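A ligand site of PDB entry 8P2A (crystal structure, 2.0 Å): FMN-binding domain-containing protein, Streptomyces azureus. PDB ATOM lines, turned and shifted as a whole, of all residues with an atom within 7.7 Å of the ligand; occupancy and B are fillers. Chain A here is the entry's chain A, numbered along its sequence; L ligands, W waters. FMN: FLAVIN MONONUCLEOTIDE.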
ATOM      1  N   THR A  12     -21.232  -1.502  15.293  1.00  0.00           N
ATOM      2  CA  THR A  12     -22.648  -1.441  15.033  1.00  0.00           C
ATOM      3  C   THR A  12     -23.302  -2.477  15.941  1.00  0.00           C
ATOM      4  O   THR A  12     -22.598  -3.237  16.555  1.00  0.00           O
ATOM      5  CB  THR A  12     -23.015  -1.644  13.565  1.00  0.00           C
ATOM      6  OG1 THR A  12     -22.982  -3.052  13.326  1.00  0.00           O
ATOM      7  CG2 THR A  12     -22.116  -0.905  12.591  1.00  0.00           C
ATOM      8  N   GLN A  13     -24.629  -2.548  15.946  1.00  0.00           N
ATOM      9  CA  GLN A  13     -25.323  -3.559  16.740  1.00  0.00           C
ATOM     10  C   GLN A  13     -25.129  -4.950  16.159  1.00  0.00           C
ATOM     11  O   GLN A  13     -25.469  -5.924  16.810  1.00  0.00           O
ATOM     12  CB  GLN A  13     -26.801  -3.179  16.848  1.00  0.00           C
ATOM     13  CG  GLN A  13     -26.990  -1.726  17.291  1.00  0.00           C
ATOM     14  CD  GLN A  13     -27.924  -1.539  18.454  1.00  0.00           C
ATOM     15  OE1 GLN A  13     -28.501  -2.488  18.986  1.00  0.00           O
ATOM     16  NE2 GLN A  13     -28.094  -0.298  18.831  1.00  0.00           N
ATOM     17  N   TYR A  14     -24.633  -5.043  14.901  1.00  0.00           N
ATOM     18  CA  TYR A  14     -24.441  -6.337  14.246  1.00  0.00           C
ATOM     19  C   TYR A  14     -22.966  -6.640  14.059  1.00  0.00           C
ATOM     20  O   TYR A  14     -22.629  -7.625  13.429  1.00  0.00           O
ATOM     21  CB  TYR A  14     -25.225  -6.398  12.939  1.00  0.00           C
ATOM     22  CG  TYR A  14     -26.718  -6.481  13.151  1.00  0.00           C
ATOM     23  CD1 TYR A  14     -27.324  -7.665  13.569  1.00  0.00           C
ATOM     24  CD2 TYR A  14     -27.526  -5.367  13.021  1.00  0.00           C
ATOM     25  CE1 TYR A  14     -28.689  -7.750  13.812  1.00  0.00           C
ATOM     26  CE2 TYR A  14     -28.882  -5.440  13.285  1.00  0.00           C
ATOM     27  CZ  TYR A  14     -29.470  -6.628  13.678  1.00  0.00           C
ATOM     28  OH  TYR A  14     -30.803  -6.627  13.878  1.00  0.00           O
ATOM     29  N   GLY A  15     -22.093  -5.820  14.659  1.00  0.00           N
ATOM     30  CA  GLY A  15     -20.668  -6.061  14.589  1.00  0.00           C
ATOM     31  C   GLY A  15     -19.947  -4.939  13.853  1.00  0.00           C
ATOM     32  O   GLY A  15     -20.565  -3.979  13.393  1.00  0.00           O
ATOM     33  N   VAL A  17     -17.799  -2.562  11.324  1.00  0.00           N
ATOM     34  CA  VAL A  17     -17.615  -2.200   9.912  1.00  0.00           C
ATOM     35  C   VAL A  17     -16.394  -1.273   9.779  1.00  0.00           C
ATOM     36  O   VAL A  17     -16.270  -0.291  10.505  1.00  0.00           O
ATOM     37  CB  VAL A  17     -18.867  -1.522   9.308  1.00  0.00           C
ATOM     38  CG1 VAL A  17     -18.765  -1.318   7.792  1.00  0.00           C
ATOM     39  CG2 VAL A  17     -20.130  -2.284   9.649  1.00  0.00           C
ATOM     40  N   ALA A  36     -16.813  -6.211   8.216  1.00  0.00           N
ATOM     41  CA  ALA A  36     -18.265  -6.177   8.035  1.00  0.00           C
ATOM     42  C   ALA A  36     -18.960  -7.224   8.916  1.00  0.00           C
ATOM     43  O   ALA A  36     -18.395  -8.275   9.186  1.00  0.00           O
ATOM     44  CB  ALA A  36     -18.627  -6.389   6.581  1.00  0.00           C
ATOM     45  N   PRO A  37     -20.217  -7.012   9.386  1.00  0.00           N
ATOM     46  CA  PRO A  37     -20.949  -8.092  10.066  1.00  0.00           C
ATOM     47  C   PRO A  37     -20.983  -9.444   9.327  1.00  0.00           C
ATOM     48  O   PRO A  37     -21.124  -9.523   8.095  1.00  0.00           O
ATOM     49  CB  PRO A  37     -22.330  -7.457  10.324  1.00  0.00           C
ATOM     50  CG  PRO A  37     -22.024  -5.978  10.481  1.00  0.00           C
ATOM     51  CD  PRO A  37     -20.916  -5.716   9.456  1.00  0.00           C
ATOM     52  N   LYS A  38     -20.799 -10.509  10.128  1.00  0.00           N
ATOM     53  CA  LYS A  38     -20.722 -11.893   9.692  1.00  0.00           C
ATOM     54  C   LYS A  38     -21.525 -12.769  10.657  1.00  0.00           C
ATOM     55  O   LYS A  38     -21.861 -12.355  11.771  1.00  0.00           O
ATOM     56  CB  LYS A  38     -19.261 -12.366   9.647  1.00  0.00           C
ATOM     57  CG  LYS A  38     -18.355 -11.746   8.585  1.00  0.00           C
ATOM     58  CD  LYS A  38     -19.031 -11.528   7.224  1.00  0.00           C
ATOM     59  CE  LYS A  38     -18.099 -11.610   6.038  1.00  0.00           C
ATOM     60  NZ  LYS A  38     -17.279 -10.390   5.872  1.00  0.00           N
ATOM     61  N   GLY A  39     -21.827 -14.001  10.215  1.00  0.00           N
ATOM     62  CA  GLY A  39     -22.535 -14.976  11.033  1.00  0.00           C
ATOM     63  C   GLY A  39     -24.045 -14.755  10.948  1.00  0.00           C
ATOM     64  O   GLY A  39     -24.503 -13.600  11.001  1.00  0.00           O
ATOM     65  N   GLY A  40     -24.803 -15.843  10.775  1.00  0.00           N
ATOM     66  CA  GLY A  40     -26.250 -15.746  10.650  1.00  0.00           C
ATOM     67  C   GLY A  40     -26.641 -14.816   9.504  1.00  0.00           C
ATOM     68  O   GLY A  40     -25.845 -14.628   8.578  1.00  0.00           O
ATOM     69  N   ARG A  41     -27.823 -14.183   9.621  1.00  0.00           N
ATOM     70  CA  ARG A  41     -28.375 -13.442   8.495  1.00  0.00           C
ATOM     71  C   ARG A  41     -27.535 -12.218   8.174  1.00  0.00           C
ATOM     72  O   ARG A  41     -27.723 -11.647   7.100  1.00  0.00           O
ATOM     73  CB  ARG A  41     -29.819 -12.960   8.674  1.00  0.00           C
ATOM     74  CG  ARG A  41     -30.454 -12.582   7.331  1.00  0.00           C
ATOM     75  CD  ARG A  41     -31.549 -11.526   7.332  1.00  0.00           C
ATOM     76  NE  ARG A  41     -32.710 -11.991   8.067  1.00  0.00           N
ATOM     77  CZ  ARG A  41     -33.342 -13.151   7.834  1.00  0.00           C
ATOM     78  NH1 ARG A  41     -33.366 -13.666   6.613  1.00  0.00           N
ATOM     79  NH2 ARG A  41     -33.965 -13.780   8.817  1.00  0.00           N
ATOM     80  N   SER A  42     -26.633 -11.815   9.085  1.00  0.00           N
ATOM     81  CA  SER A  42     -25.723 -10.711   8.874  1.00  0.00           C
ATOM     82  C   SER A  42     -24.819 -10.969   7.674  1.00  0.00           C
ATOM     83  O   SER A  42     -24.394 -10.021   7.021  1.00  0.00           O
ATOM     84  CB  SER A  42     -24.918 -10.397  10.101  1.00  0.00           C
ATOM     85  OG  SER A  42     -25.754  -9.952  11.162  1.00  0.00           O
ATOM     86  N   ASP A  43     -24.519 -12.235   7.373  1.00  0.00           N
ATOM     87  CA  ASP A  43     -23.754 -12.537   6.158  1.00  0.00           C
ATOM     88  C   ASP A  43     -24.534 -12.117   4.916  1.00  0.00           C
ATOM     89  O   ASP A  43     -23.995 -11.385   4.063  1.00  0.00           O
ATOM     90  CB  ASP A  43     -23.378 -14.009   6.046  1.00  0.00           C
ATOM     91  CG  ASP A  43     -22.196 -14.429   6.913  1.00  0.00           C
ATOM     92  OD1 ASP A  43     -21.156 -13.723   6.877  1.00  0.00           O
ATOM     93  OD2 ASP A  43     -22.322 -15.482   7.595  1.00  0.00           O
ATOM     94  N   GLN A  44     -25.788 -12.582   4.854  1.00  0.00           N
ATOM     95  CA  GLN A  44     -26.716 -12.250   3.786  1.00  0.00           C
ATOM     96  C   GLN A  44     -26.778 -10.735   3.612  1.00  0.00           C
ATOM     97  O   GLN A  44     -26.547 -10.227   2.520  1.00  0.00           O
ATOM     98  CB  GLN A  44     -28.080 -12.825   4.159  1.00  0.00           C
ATOM     99  CG  GLN A  44     -28.870 -13.379   2.990  1.00  0.00           C
ATOM    100  CD  GLN A  44     -30.009 -14.196   3.552  1.00  0.00           C
ATOM    101  OE1 GLN A  44     -30.222 -14.230   4.763  1.00  0.00           O
ATOM    102  NE2 GLN A  44     -30.729 -14.890   2.681  1.00  0.00           N
ATOM    103  N   ILE A  45     -27.022 -10.028   4.724  1.00  0.00           N
ATOM    104  CA  ILE A  45     -27.111  -8.562   4.714  1.00  0.00           C
ATOM    105  C   ILE A  45     -25.795  -7.915   4.256  1.00  0.00           C
ATOM    106  O   ILE A  45     -25.804  -6.933   3.509  1.00  0.00           O
ATOM    107  CB  ILE A  45     -27.576  -8.035   6.090  1.00  0.00           C
ATOM    108  CG1 ILE A  45     -28.841  -8.713   6.632  1.00  0.00           C
ATOM    109  CG2 ILE A  45     -27.728  -6.524   6.027  1.00  0.00           C
ATOM    110  CD1 ILE A  45     -30.009  -8.757   5.668  1.00  0.00           C
ATOM    111  N   THR A  46     -24.639  -8.438   4.719  1.00  0.00           N
ATOM    112  CA  THR A  46     -23.340  -7.894   4.345  1.00  0.00           C
ATOM    113  C   THR A  46     -23.140  -8.048   2.836  1.00  0.00           C
ATOM    114  O   THR A  46     -22.918  -7.068   2.137  1.00  0.00           O
ATOM    115  CB  THR A  46     -22.220  -8.572   5.156  1.00  0.00           C
ATOM    116  OG1 THR A  46     -22.233  -7.990   6.455  1.00  0.00           O
ATOM    117  CG2 THR A  46     -20.828  -8.358   4.588  1.00  0.00           C
ATOM    118  N   SER A  49     -25.326  -5.768   0.975  1.00  0.00           N
ATOM    119  CA  SER A  49     -25.264  -4.327   1.173  1.00  0.00           C
ATOM    120  C   SER A  49     -23.894  -3.742   0.842  1.00  0.00           C
ATOM    121  O   SER A  49     -23.819  -2.716   0.171  1.00  0.00           O
ATOM    122  CB  SER A  49     -25.680  -3.953   2.577  1.00  0.00           C
ATOM    123  OG  SER A  49     -24.755  -4.439   3.532  1.00  0.00           O
ATOM    124  N   ALA A  67     -28.150   4.994   2.516  1.00  0.00           N
ATOM    125  CA  ALA A  67     -28.202   3.740   3.265  1.00  0.00           C
ATOM    126  C   ALA A  67     -28.864   2.675   2.410  1.00  0.00           C
ATOM    127  O   ALA A  67     -29.812   2.972   1.707  1.00  0.00           O
ATOM    128  CB  ALA A  67     -28.986   3.948   4.565  1.00  0.00           C
ATOM    129  N   VAL A  68     -28.370   1.434   2.430  1.00  0.00           N
ATOM    130  CA  VAL A  68     -29.066   0.315   1.805  1.00  0.00           C
ATOM    131  C   VAL A  68     -30.222  -0.052   2.725  1.00  0.00           C
ATOM    132  O   VAL A  68     -29.968  -0.302   3.897  1.00  0.00           O
ATOM    133  CB  VAL A  68     -28.120  -0.895   1.598  1.00  0.00           C
ATOM    134  CG1 VAL A  68     -28.845  -2.122   1.060  1.00  0.00           C
ATOM    135  CG2 VAL A  68     -26.945  -0.544   0.711  1.00  0.00           C
ATOM    136  N   SER A  69     -31.463  -0.068   2.193  1.00  0.00           N
ATOM    137  CA  SER A  69     -32.658  -0.470   2.934  1.00  0.00           C
ATOM    138  C   SER A  69     -32.518  -1.910   3.395  1.00  0.00           C
ATOM    139  O   SER A  69     -32.146  -2.782   2.598  1.00  0.00           O
ATOM    140  CB  SER A  69     -33.905  -0.348   2.120  1.00  0.00           C
ATOM    141  OG  SER A  69     -34.107   0.976   1.687  1.00  0.00           O
ATOM    142  N   GLY A  70     -32.876  -2.153   4.666  1.00  0.00           N
ATOM    143  CA  GLY A  70     -32.791  -3.471   5.281  1.00  0.00           C
ATOM    144  C   GLY A  70     -31.410  -3.768   5.833  1.00  0.00           C
ATOM    145  O   GLY A  70     -31.155  -4.859   6.345  1.00  0.00           O
ATOM    146  N   ALA A  71     -30.491  -2.802   5.701  1.00  0.00           N
ATOM    147  CA  ALA A  71     -29.113  -2.946   6.122  1.00  0.00           C
ATOM    148  C   ALA A  71     -28.660  -1.597   6.676  1.00  0.00           C
ATOM    149  O   ALA A  71     -27.556  -1.130   6.378  1.00  0.00           O
ATOM    150  CB  ALA A  71     -28.264  -3.403   4.957  1.00  0.00           C
ATOM    151  N   THR A  72     -29.529  -0.981   7.482  1.00  0.00           N
ATOM    152  CA  THR A  72     -29.325   0.399   7.912  1.00  0.00           C
ATOM    153  C   THR A  72     -28.200   0.533   8.920  1.00  0.00           C
ATOM    154  O   THR A  72     -27.510   1.546   8.898  1.00  0.00           O
ATOM    155  CB  THR A  72     -30.585   1.024   8.521  1.00  0.00           C
ATOM    156  OG1 THR A  72     -31.596   1.105   7.531  1.00  0.00           O
ATOM    157  CG2 THR A  72     -30.366   2.438   9.006  1.00  0.00           C
ATOM    158  N   TYR A  73     -28.027  -0.476   9.800  1.00  0.00           N
ATOM    159  CA  TYR A  73     -26.940  -0.521  10.775  1.00  0.00           C
ATOM    160  C   TYR A  73     -25.564  -0.610  10.084  1.00  0.00           C
ATOM    161  O   TYR A  73     -24.618   0.120  10.442  1.00  0.00           O
ATOM    162  CB  TYR A  73     -27.153  -1.690  11.735  1.00  0.00           C
ATOM    163  CG  TYR A  73     -28.383  -1.498  12.568  1.00  0.00           C
ATOM    164  CD1 TYR A  73     -28.331  -0.772  13.751  1.00  0.00           C
ATOM    165  CD2 TYR A  73     -29.629  -1.855  12.092  1.00  0.00           C
ATOM    166  CE1 TYR A  73     -29.452  -0.541  14.519  1.00  0.00           C
ATOM    167  CE2 TYR A  73     -30.771  -1.619  12.835  1.00  0.00           C
ATOM    168  CZ  TYR A  73     -30.678  -0.955  14.040  1.00  0.00           C
ATOM    169  OH  TYR A  73     -31.823  -0.730  14.754  1.00  0.00           O
ATOM    170  N   THR A  74     -25.438  -1.576   9.193  1.00  0.00           N
ATOM    171  CA  THR A  74     -24.249  -1.784   8.391  1.00  0.00           C
ATOM    172  C   THR A  74     -23.945  -0.558   7.527  1.00  0.00           C
ATOM    173  O   THR A  74     -22.778  -0.206   7.384  1.00  0.00           O
ATOM    174  CB  THR A  74     -24.398  -3.018   7.500  1.00  0.00           C
ATOM    175  OG1 THR A  74     -24.398  -4.185   8.317  1.00  0.00           O
ATOM    176  CG2 THR A  74     -23.291  -3.124   6.467  1.00  0.00           C
ATOM    177  N   SER A  75     -25.000   0.076   6.963  1.00  0.00           N
ATOM    178  CA  SER A  75     -24.835   1.255   6.121  1.00  0.00           C
ATOM    179  C   SER A  75     -24.320   2.422   6.947  1.00  0.00           C
ATOM    180  O   SER A  75     -23.426   3.123   6.478  1.00  0.00           O
ATOM    181  CB  SER A  75     -26.097   1.641   5.400  1.00  0.00           C
ATOM    182  OG  SER A  75     -26.634   0.559   4.643  1.00  0.00           O
ATOM    183  N   ALA A  76     -24.869   2.625   8.163  1.00  0.00           N
ATOM    184  CA  ALA A  76     -24.480   3.706   9.044  1.00  0.00           C
ATOM    185  C   ALA A  76     -23.027   3.502   9.472  1.00  0.00           C
ATOM    186  O   ALA A  76     -22.236   4.471   9.503  1.00  0.00           O
ATOM    187  CB  ALA A  76     -25.434   3.802  10.220  1.00  0.00           C
HETATM  188  N1  FMN L   1     -29.216  -5.101   9.402  1.00  0.00           N
HETATM  189  C2  FMN L   1     -27.980  -4.615   9.143  1.00  0.00           C
HETATM  190  O2  FMN L   1     -27.854  -3.456   8.864  1.00  0.00           O
HETATM  191  N3  FMN L   1     -26.842  -5.311   9.381  1.00  0.00           N
HETATM  192  C4  FMN L   1     -26.862  -6.631   9.771  1.00  0.00           C
HETATM  193  O4  FMN L   1     -25.803  -7.243   9.908  1.00  0.00           O
HETATM  194  C4A FMN L   1     -28.163  -7.212  10.038  1.00  0.00           C
HETATM  195  N5  FMN L   1     -28.235  -8.436  10.480  1.00  0.00           N
HETATM  196  C5A FMN L   1     -29.480  -8.926  10.756  1.00  0.00           C
HETATM  197  C6  FMN L   1     -29.577 -10.235  11.270  1.00  0.00           C
HETATM  198  C7  FMN L   1     -30.789 -10.761  11.655  1.00  0.00           C
HETATM  199  C7M FMN L   1     -30.839 -12.143  12.239  1.00  0.00           C
HETATM  200  C8  FMN L   1     -31.969 -10.006  11.453  1.00  0.00           C
HETATM  201  C8M FMN L   1     -33.334 -10.580  11.790  1.00  0.00           C
HETATM  202  C9  FMN L   1     -31.889  -8.754  10.915  1.00  0.00           C
HETATM  203  C9A FMN L   1     -30.660  -8.182  10.576  1.00  0.00           C
HETATM  204  N10 FMN L   1     -30.533  -6.886  10.079  1.00  0.00           N
HETATM  205  C10 FMN L   1     -29.294  -6.348   9.847  1.00  0.00           C
HETATM  206  C1' FMN L   1     -31.702  -6.031   9.837  1.00  0.00           C
HETATM  207  C2' FMN L   1     -31.944  -5.069  10.932  1.00  0.00           C
HETATM  208  O2' FMN L   1     -32.525  -5.795  12.002  1.00  0.00           O
HETATM  209  C3' FMN L   1     -32.863  -3.953  10.443  1.00  0.00           C
HETATM  210  O3' FMN L   1     -34.097  -4.548  10.155  1.00  0.00           O
HETATM  211  C4' FMN L   1     -32.376  -3.187   9.203  1.00  0.00           C
HETATM  212  O4' FMN L   1     -30.991  -2.847   9.255  1.00  0.00           O
HETATM  213  C5' FMN L   1     -33.043  -1.840   9.100  1.00  0.00           C
HETATM  214  O5' FMN L   1     -32.809  -1.298   7.777  1.00  0.00           O
HETATM  215  P   FMN L   1     -32.955   0.295   7.582  1.00  0.00           P
HETATM  216  O1P FMN L   1     -33.618   0.518   6.218  1.00  0.00           O
HETATM  217  O2P FMN L   1     -33.671   0.842   8.841  1.00  0.00           O
HETATM  218  O   HOH W   1     -34.979  -6.565  12.183  1.00  0.00           O
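An oxygen (O4') of the ligand lies within hydrogen-bond range of the backbone NH (N) of Thr 72 (3.0 Å).
OG1 of Thr 72 is covalently linked to P of the ligand.
OH of Tyr 14 sits at hydrogen-bond distance from O2' of the ligand.
O2 of the ligand is in hydrogen-bond range of N of Thr 74 (3.1 Å).
OG1 of Thr 74 lies within hydrogen-bond range of N3 of the ligand (2.9 Å).
The backbone NH (N) of Ala 71 lies within hydrogen-bond range of an oxygen (O5') of the ligand (3.5 Å).
OG of Ser 42 is in hydrogen-bond range of O4 of the ligand.
N of Tyr 73 is in hydrogen-bond range of O2 of the ligand (3.1 Å).
The backbone NH (N) of Gly 70 sits at hydrogen-bond distance from an oxygen (O1P) of the ligand (3.2 Å).
N of Tyr 14 sits at hydrogen-bond distance from OG1 of Thr 12 (3.0 Å).
O of Ala 71 is in hydrogen-bond range of OG of Ser 75 (2.6 Å).
OG1 of Thr 46 lies within hydrogen-bond range of O of Ser 42, 3.0 Å away.
The side-chain hydroxyl of Thr 46 sits at hydrogen-bond distance from the backbone carbonyl oxygen of Pro 37.
OG of Ser 49 sits at hydrogen-bond distance from O of Ile 45 (2.7 Å).
Merely in contact with the ligand: Pro 37 (3.5 Å), Ser 69 (3.6 Å), Ile 45 (3.7 Å) and Arg 41 (3.8 Å).
Hydrophobic or aromatic side chains that line the ligand: Tyr 14, Pro 37, Ile 45, Ala 71 and Tyr 73.
Within 4 Å of the ligand: Tyr 14, Pro 37, Arg 41, Ser 42, Ile 45, Ser 69, Gly 70, Ala 71, Thr 72, Tyr 73 and Thr 74.
The nearest printed residue that does not touch the ligand is Val 68 (4.4 Å).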
